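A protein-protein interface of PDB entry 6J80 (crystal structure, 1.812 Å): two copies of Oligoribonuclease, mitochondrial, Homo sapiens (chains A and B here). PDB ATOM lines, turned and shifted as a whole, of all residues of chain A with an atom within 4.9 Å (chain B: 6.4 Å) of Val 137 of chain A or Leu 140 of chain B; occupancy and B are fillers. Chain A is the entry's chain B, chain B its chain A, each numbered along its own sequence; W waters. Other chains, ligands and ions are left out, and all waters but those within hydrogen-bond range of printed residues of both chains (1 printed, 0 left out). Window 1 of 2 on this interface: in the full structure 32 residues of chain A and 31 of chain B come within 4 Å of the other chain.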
ATOM      1  N   MET A   8      -8.292 -14.699  14.659  1.00  0.00           N
ATOM      2  CA  MET A   8      -8.000 -14.068  15.939  1.00  0.00           C
ATOM      3  C   MET A   8      -6.973 -12.965  15.744  1.00  0.00           C
ATOM      4  O   MET A   8      -6.004 -13.131  14.981  1.00  0.00           O
ATOM      5  CB  MET A   8      -7.441 -15.072  16.961  1.00  0.00           C
ATOM      6  CG  MET A   8      -8.284 -16.316  17.178  1.00  0.00           C
ATOM      7  SD  MET A   8      -7.387 -17.417  18.292  1.00  0.00           S
ATOM      8  CE  MET A   8      -8.426 -18.887  18.201  1.00  0.00           C
ATOM      9  N   ILE A 132     -10.217 -13.590  23.571  1.00  0.00           N
ATOM     10  CA  ILE A 132      -9.681 -14.917  23.824  1.00  0.00           C
ATOM     11  C   ILE A 132      -8.529 -14.719  24.789  1.00  0.00           C
ATOM     12  O   ILE A 132      -7.411 -14.397  24.381  1.00  0.00           O
ATOM     13  CB  ILE A 132      -9.245 -15.612  22.536  1.00  0.00           C
ATOM     14  CG1 ILE A 132     -10.493 -15.795  21.657  1.00  0.00           C
ATOM     15  CG2 ILE A 132      -8.544 -16.968  22.875  1.00  0.00           C
ATOM     16  CD1 ILE A 132     -10.263 -16.547  20.379  1.00  0.00           C
ATOM     17  N   ASP A 133      -8.808 -14.913  26.072  1.00  0.00           N
ATOM     18  CA  ASP A 133      -7.845 -14.638  27.143  1.00  0.00           C
ATOM     19  C   ASP A 133      -7.136 -15.944  27.456  1.00  0.00           C
ATOM     20  O   ASP A 133      -7.699 -16.830  28.099  1.00  0.00           O
ATOM     21  CB  ASP A 133      -8.552 -14.068  28.373  1.00  0.00           C
ATOM     22  CG  ASP A 133      -7.598 -13.860  29.561  1.00  0.00           C
ATOM     23  OD1 ASP A 133      -6.364 -13.918  29.382  1.00  0.00           O
ATOM     24  OD2 ASP A 133      -8.079 -13.673  30.695  1.00  0.00           O
ATOM     25  N   VAL A 134      -5.890 -16.067  26.997  1.00  0.00           N
ATOM     26  CA  VAL A 134      -5.160 -17.313  27.199  1.00  0.00           C
ATOM     27  C   VAL A 134      -4.959 -17.550  28.689  1.00  0.00           C
ATOM     28  O   VAL A 134      -4.869 -18.696  29.139  1.00  0.00           O
ATOM     29  CB  VAL A 134      -3.830 -17.280  26.409  1.00  0.00           C
ATOM     30  CG1 VAL A 134      -3.006 -18.567  26.663  1.00  0.00           C
ATOM     31  CG2 VAL A 134      -4.130 -17.132  24.895  1.00  0.00           C
ATOM     32  N   SER A 135      -4.932 -16.479  29.489  1.00  0.00           N
ATOM     33  CA  SER A 135      -4.729 -16.666  30.927  1.00  0.00           C
ATOM     34  C   SER A 135      -5.956 -17.237  31.621  1.00  0.00           C
ATOM     35  O   SER A 135      -5.827 -17.831  32.704  1.00  0.00           O
ATOM     36  CB  SER A 135      -4.309 -15.341  31.566  1.00  0.00           C
ATOM     37  OG  SER A 135      -2.962 -15.084  31.190  1.00  0.00           O
ATOM     38  N   THR A 136      -7.140 -17.117  31.011  1.00  0.00           N
ATOM     39  CA  THR A 136      -8.287 -17.875  31.500  1.00  0.00           C
ATOM     40  C   THR A 136      -8.010 -19.369  31.385  1.00  0.00           C
ATOM     41  O   THR A 136      -8.263 -20.148  32.325  1.00  0.00           O
ATOM     42  CB  THR A 136      -9.546 -17.508  30.708  1.00  0.00           C
ATOM     43  OG1 THR A 136     -10.003 -16.199  31.071  1.00  0.00           O
ATOM     44  CG2 THR A 136     -10.669 -18.517  30.966  1.00  0.00           C
ATOM     45  N   VAL A 137      -7.484 -19.784  30.227  1.00  0.00           N
ATOM     46  CA  VAL A 137      -7.207 -21.201  30.022  1.00  0.00           C
ATOM     47  C   VAL A 137      -6.080 -21.634  30.940  1.00  0.00           C
ATOM     48  O   VAL A 137      -6.096 -22.748  31.471  1.00  0.00           O
ATOM     49  CB  VAL A 137      -6.893 -21.492  28.539  1.00  0.00           C
ATOM     50  CG1 VAL A 137      -6.808 -23.024  28.304  1.00  0.00           C
ATOM     51  CG2 VAL A 137      -8.000 -20.896  27.638  1.00  0.00           C
ATOM     52  N   LYS A 138      -5.092 -20.756  31.148  1.00  0.00           N
ATOM     53  CA  LYS A 138      -4.045 -20.998  32.136  1.00  0.00           C
ATOM     54  C   LYS A 138      -4.631 -21.296  33.519  1.00  0.00           C
ATOM     55  O   LYS A 138      -4.233 -22.267  34.172  1.00  0.00           O
ATOM     56  CB  LYS A 138      -3.105 -19.792  32.196  1.00  0.00           C
ATOM     57  CG  LYS A 138      -1.954 -19.919  33.207  1.00  0.00           C
ATOM     58  CD  LYS A 138      -1.496 -18.533  33.655  1.00  0.00           C
ATOM     59  CE  LYS A 138      -0.985 -17.693  32.495  1.00  0.00           C
ATOM     60  NZ  LYS A 138       0.316 -18.217  31.941  1.00  0.00           N
ATOM     61  N   GLU A 139      -5.567 -20.457  33.987  1.00  0.00           N
ATOM     62  CA  GLU A 139      -6.133 -20.643  35.331  1.00  0.00           C
ATOM     63  C   GLU A 139      -6.935 -21.939  35.423  1.00  0.00           C
ATOM     64  O   GLU A 139      -6.895 -22.643  36.452  1.00  0.00           O
ATOM     65  CB  GLU A 139      -6.983 -19.426  35.715  1.00  0.00           C
ATOM     66  CG  GLU A 139      -6.114 -18.204  36.053  1.00  0.00           C
ATOM     67  CD  GLU A 139      -5.253 -18.458  37.280  1.00  0.00           C
ATOM     68  OE1 GLU A 139      -5.813 -18.899  38.302  1.00  0.00           O
ATOM     69  OE2 GLU A 139      -4.021 -18.259  37.219  1.00  0.00           O
ATOM     70  N   LEU A 140      -7.621 -22.306  34.333  1.00  0.00           N
ATOM     71  CA  LEU A 140      -8.338 -23.575  34.328  1.00  0.00           C
ATOM     72  C   LEU A 140      -7.383 -24.759  34.277  1.00  0.00           C
ATOM     73  O   LEU A 140      -7.658 -25.799  34.889  1.00  0.00           O
ATOM     74  CB  LEU A 140      -9.314 -23.639  33.153  1.00  0.00           C
ATOM     75  CG  LEU A 140     -10.393 -22.559  33.231  1.00  0.00           C
ATOM     76  CD1 LEU A 140     -11.219 -22.627  31.947  1.00  0.00           C
ATOM     77  CD2 LEU A 140     -11.275 -22.736  34.497  1.00  0.00           C
ATOM     78  N   CYS A 141      -6.273 -24.634  33.542  1.00  0.00           N
ATOM     79  CA  CYS A 141      -5.274 -25.696  33.502  1.00  0.00           C
ATOM     80  C   CYS A 141      -4.684 -25.927  34.881  1.00  0.00           C
ATOM     81  O   CYS A 141      -4.536 -27.069  35.323  1.00  0.00           O
ATOM     82  CB  CYS A 141      -4.164 -25.340  32.506  1.00  0.00           C
ATOM     83  SG  CYS A 141      -2.991 -26.690  32.184  1.00  0.00           S
ATOM     84  N   LEU A 172      -1.266 -21.278  24.326  1.00  0.00           N
ATOM     85  CA  LEU A 172      -2.597 -21.765  23.960  1.00  0.00           C
ATOM     86  C   LEU A 172      -2.509 -23.063  23.155  1.00  0.00           C
ATOM     87  O   LEU A 172      -3.317 -23.981  23.355  1.00  0.00           O
ATOM     88  CB  LEU A 172      -3.373 -20.686  23.195  1.00  0.00           C
ATOM     89  CG  LEU A 172      -4.830 -21.068  22.865  1.00  0.00           C
ATOM     90  CD1 LEU A 172      -5.627 -21.367  24.141  1.00  0.00           C
ATOM     91  CD2 LEU A 172      -5.523 -19.966  22.088  1.00  0.00           C
ATOM     92  N   TYR A 175      -2.098 -25.832  25.562  1.00  0.00           N
ATOM     93  CA  TYR A 175      -3.343 -26.239  26.215  1.00  0.00           C
ATOM     94  C   TYR A 175      -4.211 -27.050  25.268  1.00  0.00           C
ATOM     95  O   TYR A 175      -4.785 -28.074  25.660  1.00  0.00           O
ATOM     96  CB  TYR A 175      -4.125 -25.035  26.738  1.00  0.00           C
ATOM     97  CG  TYR A 175      -3.373 -24.264  27.795  1.00  0.00           C
ATOM     98  CD1 TYR A 175      -2.687 -24.926  28.814  1.00  0.00           C
ATOM     99  CD2 TYR A 175      -3.328 -22.879  27.756  1.00  0.00           C
ATOM    100  CE1 TYR A 175      -1.969 -24.210  29.775  1.00  0.00           C
ATOM    101  CE2 TYR A 175      -2.642 -22.143  28.725  1.00  0.00           C
ATOM    102  CZ  TYR A 175      -1.952 -22.820  29.711  1.00  0.00           C
ATOM    103  OH  TYR A 175      -1.259 -22.120  30.641  1.00  0.00           O
ATOM    104  N   ILE A 179      -4.910 -30.482  27.181  1.00  0.00           N
ATOM    105  CA  ILE A 179      -6.033 -30.518  28.109  1.00  0.00           C
ATOM    106  C   ILE A 179      -7.387 -30.440  27.424  1.00  0.00           C
ATOM    107  O   ILE A 179      -8.411 -30.542  28.100  1.00  0.00           O
ATOM    108  CB  ILE A 179      -5.926 -29.434  29.206  1.00  0.00           C
ATOM    109  CG1 ILE A 179      -6.180 -28.025  28.643  1.00  0.00           C
ATOM    110  CG2 ILE A 179      -4.565 -29.476  29.897  1.00  0.00           C
ATOM    111  CD1 ILE A 179      -6.195 -26.963  29.774  1.00  0.00           C
ATOM    112  N   PHE A 180      -7.440 -30.267  26.110  1.00  0.00           N
ATOM    113  CA  PHE A 180      -8.700 -30.369  25.394  1.00  0.00           C
ATOM    114  C   PHE A 180      -8.877 -31.766  24.804  1.00  0.00           C
ATOM    115  O   PHE A 180      -7.917 -32.500  24.564  1.00  0.00           O
ATOM    116  CB  PHE A 180      -8.799 -29.298  24.303  1.00  0.00           C
ATOM    117  CG  PHE A 180      -9.024 -27.907  24.861  1.00  0.00           C
ATOM    118  CD1 PHE A 180      -7.978 -27.205  25.443  1.00  0.00           C
ATOM    119  CD2 PHE A 180     -10.284 -27.334  24.829  1.00  0.00           C
ATOM    120  CE1 PHE A 180      -8.192 -25.928  25.989  1.00  0.00           C
ATOM    121  CE2 PHE A 180     -10.509 -26.059  25.366  1.00  0.00           C
ATOM    122  CZ  PHE A 180      -9.464 -25.365  25.950  1.00  0.00           C
ATOM    123  N   ILE B 131      -8.492 -13.244  35.182  1.00  0.00           N
ATOM    124  CA  ILE B 131      -9.916 -13.538  35.208  1.00  0.00           C
ATOM    125  C   ILE B 131     -10.139 -14.930  34.648  1.00  0.00           C
ATOM    126  O   ILE B 131      -9.300 -15.486  33.932  1.00  0.00           O
ATOM    127  CB  ILE B 131     -10.764 -12.517  34.402  1.00  0.00           C
ATOM    128  CG1 ILE B 131     -10.340 -12.542  32.926  1.00  0.00           C
ATOM    129  CG2 ILE B 131     -10.627 -11.127  34.998  1.00  0.00           C
ATOM    130  CD1 ILE B 131     -11.106 -11.553  32.039  1.00  0.00           C
ATOM    131  N   SER B 135     -16.550 -16.636  28.383  1.00  0.00           N
ATOM    132  CA  SER B 135     -16.717 -16.348  26.955  1.00  0.00           C
ATOM    133  C   SER B 135     -15.462 -16.658  26.147  1.00  0.00           C
ATOM    134  O   SER B 135     -15.576 -16.906  24.938  1.00  0.00           O
ATOM    135  CB  SER B 135     -17.123 -14.883  26.753  1.00  0.00           C
ATOM    136  OG  SER B 135     -18.463 -14.708  27.180  1.00  0.00           O
ATOM    137  N   THR B 136     -14.275 -16.657  26.780  1.00  0.00           N
ATOM    138  CA  THR B 136     -13.071 -17.158  26.099  1.00  0.00           C
ATOM    139  C   THR B 136     -13.242 -18.641  25.744  1.00  0.00           C
ATOM    140  O   THR B 136     -12.926 -19.080  24.623  1.00  0.00           O
ATOM    141  CB  THR B 136     -11.818 -16.975  26.971  1.00  0.00           C
ATOM    142  OG1 THR B 136     -11.388 -15.611  26.982  1.00  0.00           O
ATOM    143  CG2 THR B 136     -10.647 -17.807  26.421  1.00  0.00           C
ATOM    144  N   VAL B 137     -13.743 -19.429  26.700  1.00  0.00           N
ATOM    145  CA  VAL B 137     -13.935 -20.852  26.445  1.00  0.00           C
ATOM    146  C   VAL B 137     -15.035 -21.050  25.409  1.00  0.00           C
ATOM    147  O   VAL B 137     -14.955 -21.947  24.565  1.00  0.00           O
ATOM    148  CB  VAL B 137     -14.226 -21.602  27.760  1.00  0.00           C
ATOM    149  CG1 VAL B 137     -14.213 -23.128  27.525  1.00  0.00           C
ATOM    150  CG2 VAL B 137     -13.173 -21.238  28.819  1.00  0.00           C
ATOM    151  N   LYS B 138     -16.065 -20.198  25.442  1.00  0.00           N
ATOM    152  CA  LYS B 138     -17.092 -20.207  24.398  1.00  0.00           C
ATOM    153  C   LYS B 138     -16.490 -20.008  23.004  1.00  0.00           C
ATOM    154  O   LYS B 138     -16.817 -20.747  22.062  1.00  0.00           O
ATOM    155  CB  LYS B 138     -18.136 -19.123  24.721  1.00  0.00           C
ATOM    156  CG  LYS B 138     -19.237 -18.935  23.688  1.00  0.00           C
ATOM    157  CD  LYS B 138     -19.920 -17.567  23.895  1.00  0.00           C
ATOM    158  CE  LYS B 138     -21.230 -17.468  23.116  1.00  0.00           C
ATOM    159  NZ  LYS B 138     -22.282 -18.382  23.644  1.00  0.00           N
ATOM    160  N   GLU B 139     -15.608 -19.011  22.845  1.00  0.00           N
ATOM    161  CA  GLU B 139     -15.039 -18.739  21.522  1.00  0.00           C
ATOM    162  C   GLU B 139     -14.157 -19.896  21.041  1.00  0.00           C
ATOM    163  O   GLU B 139     -14.132 -20.226  19.837  1.00  0.00           O
ATOM    164  CB  GLU B 139     -14.249 -17.430  21.558  1.00  0.00           C
ATOM    165  CG  GLU B 139     -15.160 -16.192  21.623  1.00  0.00           C
ATOM    166  CD  GLU B 139     -16.067 -16.101  20.405  1.00  0.00           C
ATOM    167  OE1 GLU B 139     -17.303 -15.944  20.555  1.00  0.00           O
ATOM    168  OE2 GLU B 139     -15.533 -16.217  19.288  1.00  0.00           O
ATOM    169  N   LEU B 140     -13.447 -20.543  21.979  1.00  0.00           N
ATOM    170  CA  LEU B 140     -12.670 -21.721  21.610  1.00  0.00           C
ATOM    171  C   LEU B 140     -13.571 -22.901  21.264  1.00  0.00           C
ATOM    172  O   LEU B 140     -13.281 -23.647  20.322  1.00  0.00           O
ATOM    173  CB  LEU B 140     -11.701 -22.092  22.732  1.00  0.00           C
ATOM    174  CG  LEU B 140     -10.656 -21.015  23.022  1.00  0.00           C
ATOM    175  CD1 LEU B 140      -9.815 -21.460  24.205  1.00  0.00           C
ATOM    176  CD2 LEU B 140      -9.775 -20.712  21.803  1.00  0.00           C
ATOM    177  N   CYS B 141     -14.663 -23.090  22.006  1.00  0.00           N
ATOM    178  CA  CYS B 141     -15.603 -24.162  21.694  1.00  0.00           C
ATOM    179  C   CYS B 141     -16.184 -23.992  20.301  1.00  0.00           C
ATOM    180  O   CYS B 141     -16.309 -24.958  19.538  1.00  0.00           O
ATOM    181  CB  CYS B 141     -16.739 -24.171  22.718  1.00  0.00           C
ATOM    182  SG  CYS B 141     -17.815 -25.648  22.587  1.00  0.00           S
ATOM    183  N   ARG B 142     -16.599 -22.771  19.982  1.00  0.00           N
ATOM    184  CA  ARG B 142     -17.198 -22.487  18.680  1.00  0.00           C
ATOM    185  C   ARG B 142     -16.246 -22.843  17.545  1.00  0.00           C
ATOM    186  O   ARG B 142     -16.672 -23.378  16.505  1.00  0.00           O
ATOM    187  CB  ARG B 142     -17.583 -21.010  18.616  1.00  0.00           C
ATOM    188  CG  ARG B 142     -18.296 -20.610  17.352  1.00  0.00           C
ATOM    189  CD  ARG B 142     -18.996 -19.282  17.574  1.00  0.00           C
ATOM    190  NE  ARG B 142     -18.054 -18.172  17.576  1.00  0.00           N
ATOM    191  CZ  ARG B 142     -17.528 -17.660  16.469  1.00  0.00           C
ATOM    192  NH1 ARG B 142     -17.850 -18.175  15.292  1.00  0.00           N
ATOM    193  NH2 ARG B 142     -16.682 -16.640  16.542  1.00  0.00           N
ATOM    194  N   ARG B 143     -14.947 -22.572  17.734  1.00  0.00           N
ATOM    195  CA  ARG B 143     -13.968 -22.867  16.691  1.00  0.00           C
ATOM    196  C   ARG B 143     -13.579 -24.346  16.636  1.00  0.00           C
ATOM    197  O   ARG B 143     -13.541 -24.948  15.555  1.00  0.00           O
ATOM    198  CB  ARG B 143     -12.721 -22.020  16.909  1.00  0.00           C
ATOM    199  CG  ARG B 143     -12.949 -20.547  16.660  1.00  0.00           C
ATOM    200  CD  ARG B 143     -11.753 -19.722  17.151  1.00  0.00           C
ATOM    201  NE  ARG B 143     -11.793 -18.357  16.619  1.00  0.00           N
ATOM    202  CZ  ARG B 143     -12.611 -17.417  17.074  1.00  0.00           C
ATOM    203  NH1 ARG B 143     -13.429 -17.681  18.073  1.00  0.00           N
ATOM    204  NH2 ARG B 143     -12.593 -16.207  16.531  1.00  0.00           N
ATOM    205  N   TRP B 144     -13.240 -24.928  17.779  1.00  0.00           N
ATOM    206  CA  TRP B 144     -12.606 -26.236  17.830  1.00  0.00           C
ATOM    207  C   TRP B 144     -13.583 -27.386  18.044  1.00  0.00           C
ATOM    208  O   TRP B 144     -13.226 -28.534  17.754  1.00  0.00           O
ATOM    209  CB  TRP B 144     -11.566 -26.263  18.958  1.00  0.00           C
ATOM    210  CG  TRP B 144     -10.441 -25.269  18.822  1.00  0.00           C
ATOM    211  CD1 TRP B 144     -10.074 -24.565  17.712  1.00  0.00           C
ATOM    212  CD2 TRP B 144      -9.544 -24.895  19.856  1.00  0.00           C
ATOM    213  NE1 TRP B 144      -8.989 -23.748  18.005  1.00  0.00           N
ATOM    214  CE2 TRP B 144      -8.645 -23.948  19.317  1.00  0.00           C
ATOM    215  CE3 TRP B 144      -9.412 -25.273  21.200  1.00  0.00           C
ATOM    216  CZ2 TRP B 144      -7.625 -23.377  20.072  1.00  0.00           C
ATOM    217  CZ3 TRP B 144      -8.399 -24.692  21.958  1.00  0.00           C
ATOM    218  CH2 TRP B 144      -7.515 -23.769  21.388  1.00  0.00           C
ATOM    219  N   TYR B 145     -14.791 -27.108  18.549  1.00  0.00           N
ATOM    220  CA  TYR B 145     -15.775 -28.143  18.883  1.00  0.00           C
ATOM    221  C   TYR B 145     -17.157 -27.683  18.424  1.00  0.00           C
ATOM    222  O   TYR B 145     -18.075 -27.520  19.231  1.00  0.00           O
ATOM    223  CB  TYR B 145     -15.748 -28.451  20.389  1.00  0.00           C
ATOM    224  CG  TYR B 145     -14.389 -28.993  20.803  1.00  0.00           C
ATOM    225  CD1 TYR B 145     -14.093 -30.348  20.686  1.00  0.00           C
ATOM    226  CD2 TYR B 145     -13.393 -28.144  21.273  1.00  0.00           C
ATOM    227  CE1 TYR B 145     -12.843 -30.830  21.023  1.00  0.00           C
ATOM    228  CE2 TYR B 145     -12.141 -28.616  21.601  1.00  0.00           C
ATOM    229  CZ  TYR B 145     -11.867 -29.964  21.481  1.00  0.00           C
ATOM    230  OH  TYR B 145     -10.612 -30.449  21.801  1.00  0.00           O
ATOM    231  N   ILE B 179     -15.684 -30.648  26.200  1.00  0.00           N
ATOM    232  CA  ILE B 179     -14.573 -30.349  25.298  1.00  0.00           C
ATOM    233  C   ILE B 179     -13.219 -30.428  25.991  1.00  0.00           C
ATOM    234  O   ILE B 179     -12.181 -30.303  25.331  1.00  0.00           O
ATOM    235  CB  ILE B 179     -14.743 -28.982  24.602  1.00  0.00           C
ATOM    236  CG1 ILE B 179     -14.412 -27.827  25.554  1.00  0.00           C
ATOM    237  CG2 ILE B 179     -16.151 -28.821  23.975  1.00  0.00           C
ATOM    238  CD1 ILE B 179     -14.463 -26.439  24.839  1.00  0.00           C
ATOM    239  N   PHE B 180     -13.190 -30.621  27.307  1.00  0.00           N
ATOM    240  CA  PHE B 180     -11.899 -30.830  27.940  1.00  0.00           C
ATOM    241  C   PHE B 180     -11.586 -32.321  28.055  1.00  0.00           C
ATOM    242  O   PHE B 180     -12.471 -33.171  28.016  1.00  0.00           O
ATOM    243  CB  PHE B 180     -11.834 -30.160  29.317  1.00  0.00           C
ATOM    244  CG  PHE B 180     -11.661 -28.663  29.241  1.00  0.00           C
ATOM    245  CD1 PHE B 180     -12.745 -27.845  28.951  1.00  0.00           C
ATOM    246  CD2 PHE B 180     -10.413 -28.085  29.447  1.00  0.00           C
ATOM    247  CE1 PHE B 180     -12.599 -26.438  28.874  1.00  0.00           C
ATOM    248  CE2 PHE B 180     -10.244 -26.702  29.365  1.00  0.00           C
ATOM    249  CZ  PHE B 180     -11.348 -25.877  29.074  1.00  0.00           C
HETATM  250  O   HOH W   1      -6.747 -13.175  32.766  1.00  0.00           O
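Of the 15 printed residues of chain A, 8 touch a printed residue of chain B. Printed residues of chain B that touch a printed residue of chain A: Ile 131, Thr 136, Val 137, Leu 140, Arg 143, Tyr 145, Ile 179 and Phe 180. Hydrophobic or aromatic side chains of chain B within 4 Å of the printed part of chain A: Ile 131, Val 137, Leu 140, Tyr 145 and Phe 180. Among the printed residues, 11 pairs touch across the chains.
Water W1 bridges OD2 of Asp 133 of chain A (2.5 Å) and N of Ile 131 of chain B (3.0 Å).
Of the printed residues of chain B, Met 8 of chain A touches Arg 143 (3.6 Å). Printed residues of chain B within 4 Å of Ile 132 of chain A: Thr 136. Of chain B, only Leu 140 comes within 4 Å of Val 137 of chain A. Of chain A, only Val 137 (3.9 Å) comes within 4 Å of Leu 140 of chain B. The nearest printed residue of chain A that does not touch Arg 143 of chain B is Ile 132 of chain A (4.1 Å).
The backbone carbonyl oxygen (O) of Tyr 175 of chain A lies close to the backbone NH (N) of Phe 180 of chain A, at 3.5 Å. OD2 of Asp 133 of chain A lies within hydrogen-bond range of OG1 of Thr 136 of chain A. The side-chain carboxylate (OE2) of Glu 139 of chain B is in salt-bridge range of the guanidinium group (NH1) of Arg 143 of chain B (2.8 Å). OD1 of Asp 133 of chain A sits at hydrogen-bond distance from N of Ser 135 of chain A (2.9 Å).
Val 137 of chain A touches Leu 140 of chain B, and with the chains exchanged Leu 140 of chain A touches Val 137 of chain B. Ile 179 of chain A touches Phe 180 of chain B, and with the chains exchanged Phe 180 of chain A touches Ile 179 of chain B. Phe 180 of chain B touches its own counterpart, Phe 180 of chain A.
The side-chain hydroxyl of Thr 136 of chain B lies within hydrogen-bond range of the backbone NH of Asp 133 of chain A (2.8 Å). OG1 of Thr 136 of chain A lies within hydrogen-bond range of O of Ile 131 of chain B (3.0 Å).
Among the printed residues, merely in contact across the chains: Phe 180 of chain A with Tyr 145 of chain B (3.3 Å), Asp 133 of chain A with Ile 131 of chain B (3.4 Å), Ile 179 of chain A with Phe 180 of chain B (3.4 Å), Phe 180 of chain A with Ile 179 of chain B (3.5 Å), Met 8 of chain A with Arg 143 of chain B (3.6 Å), Ile 132 of chain A with Thr 136 of chain B (3.7 Å), Phe 180 of chain A with Phe 180 of chain B (3.7 Å), Val 137 of chain A with Leu 140 of chain B (3.9 Å) and Leu 140 of chain A with Val 137 of chain B (3.9 Å).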
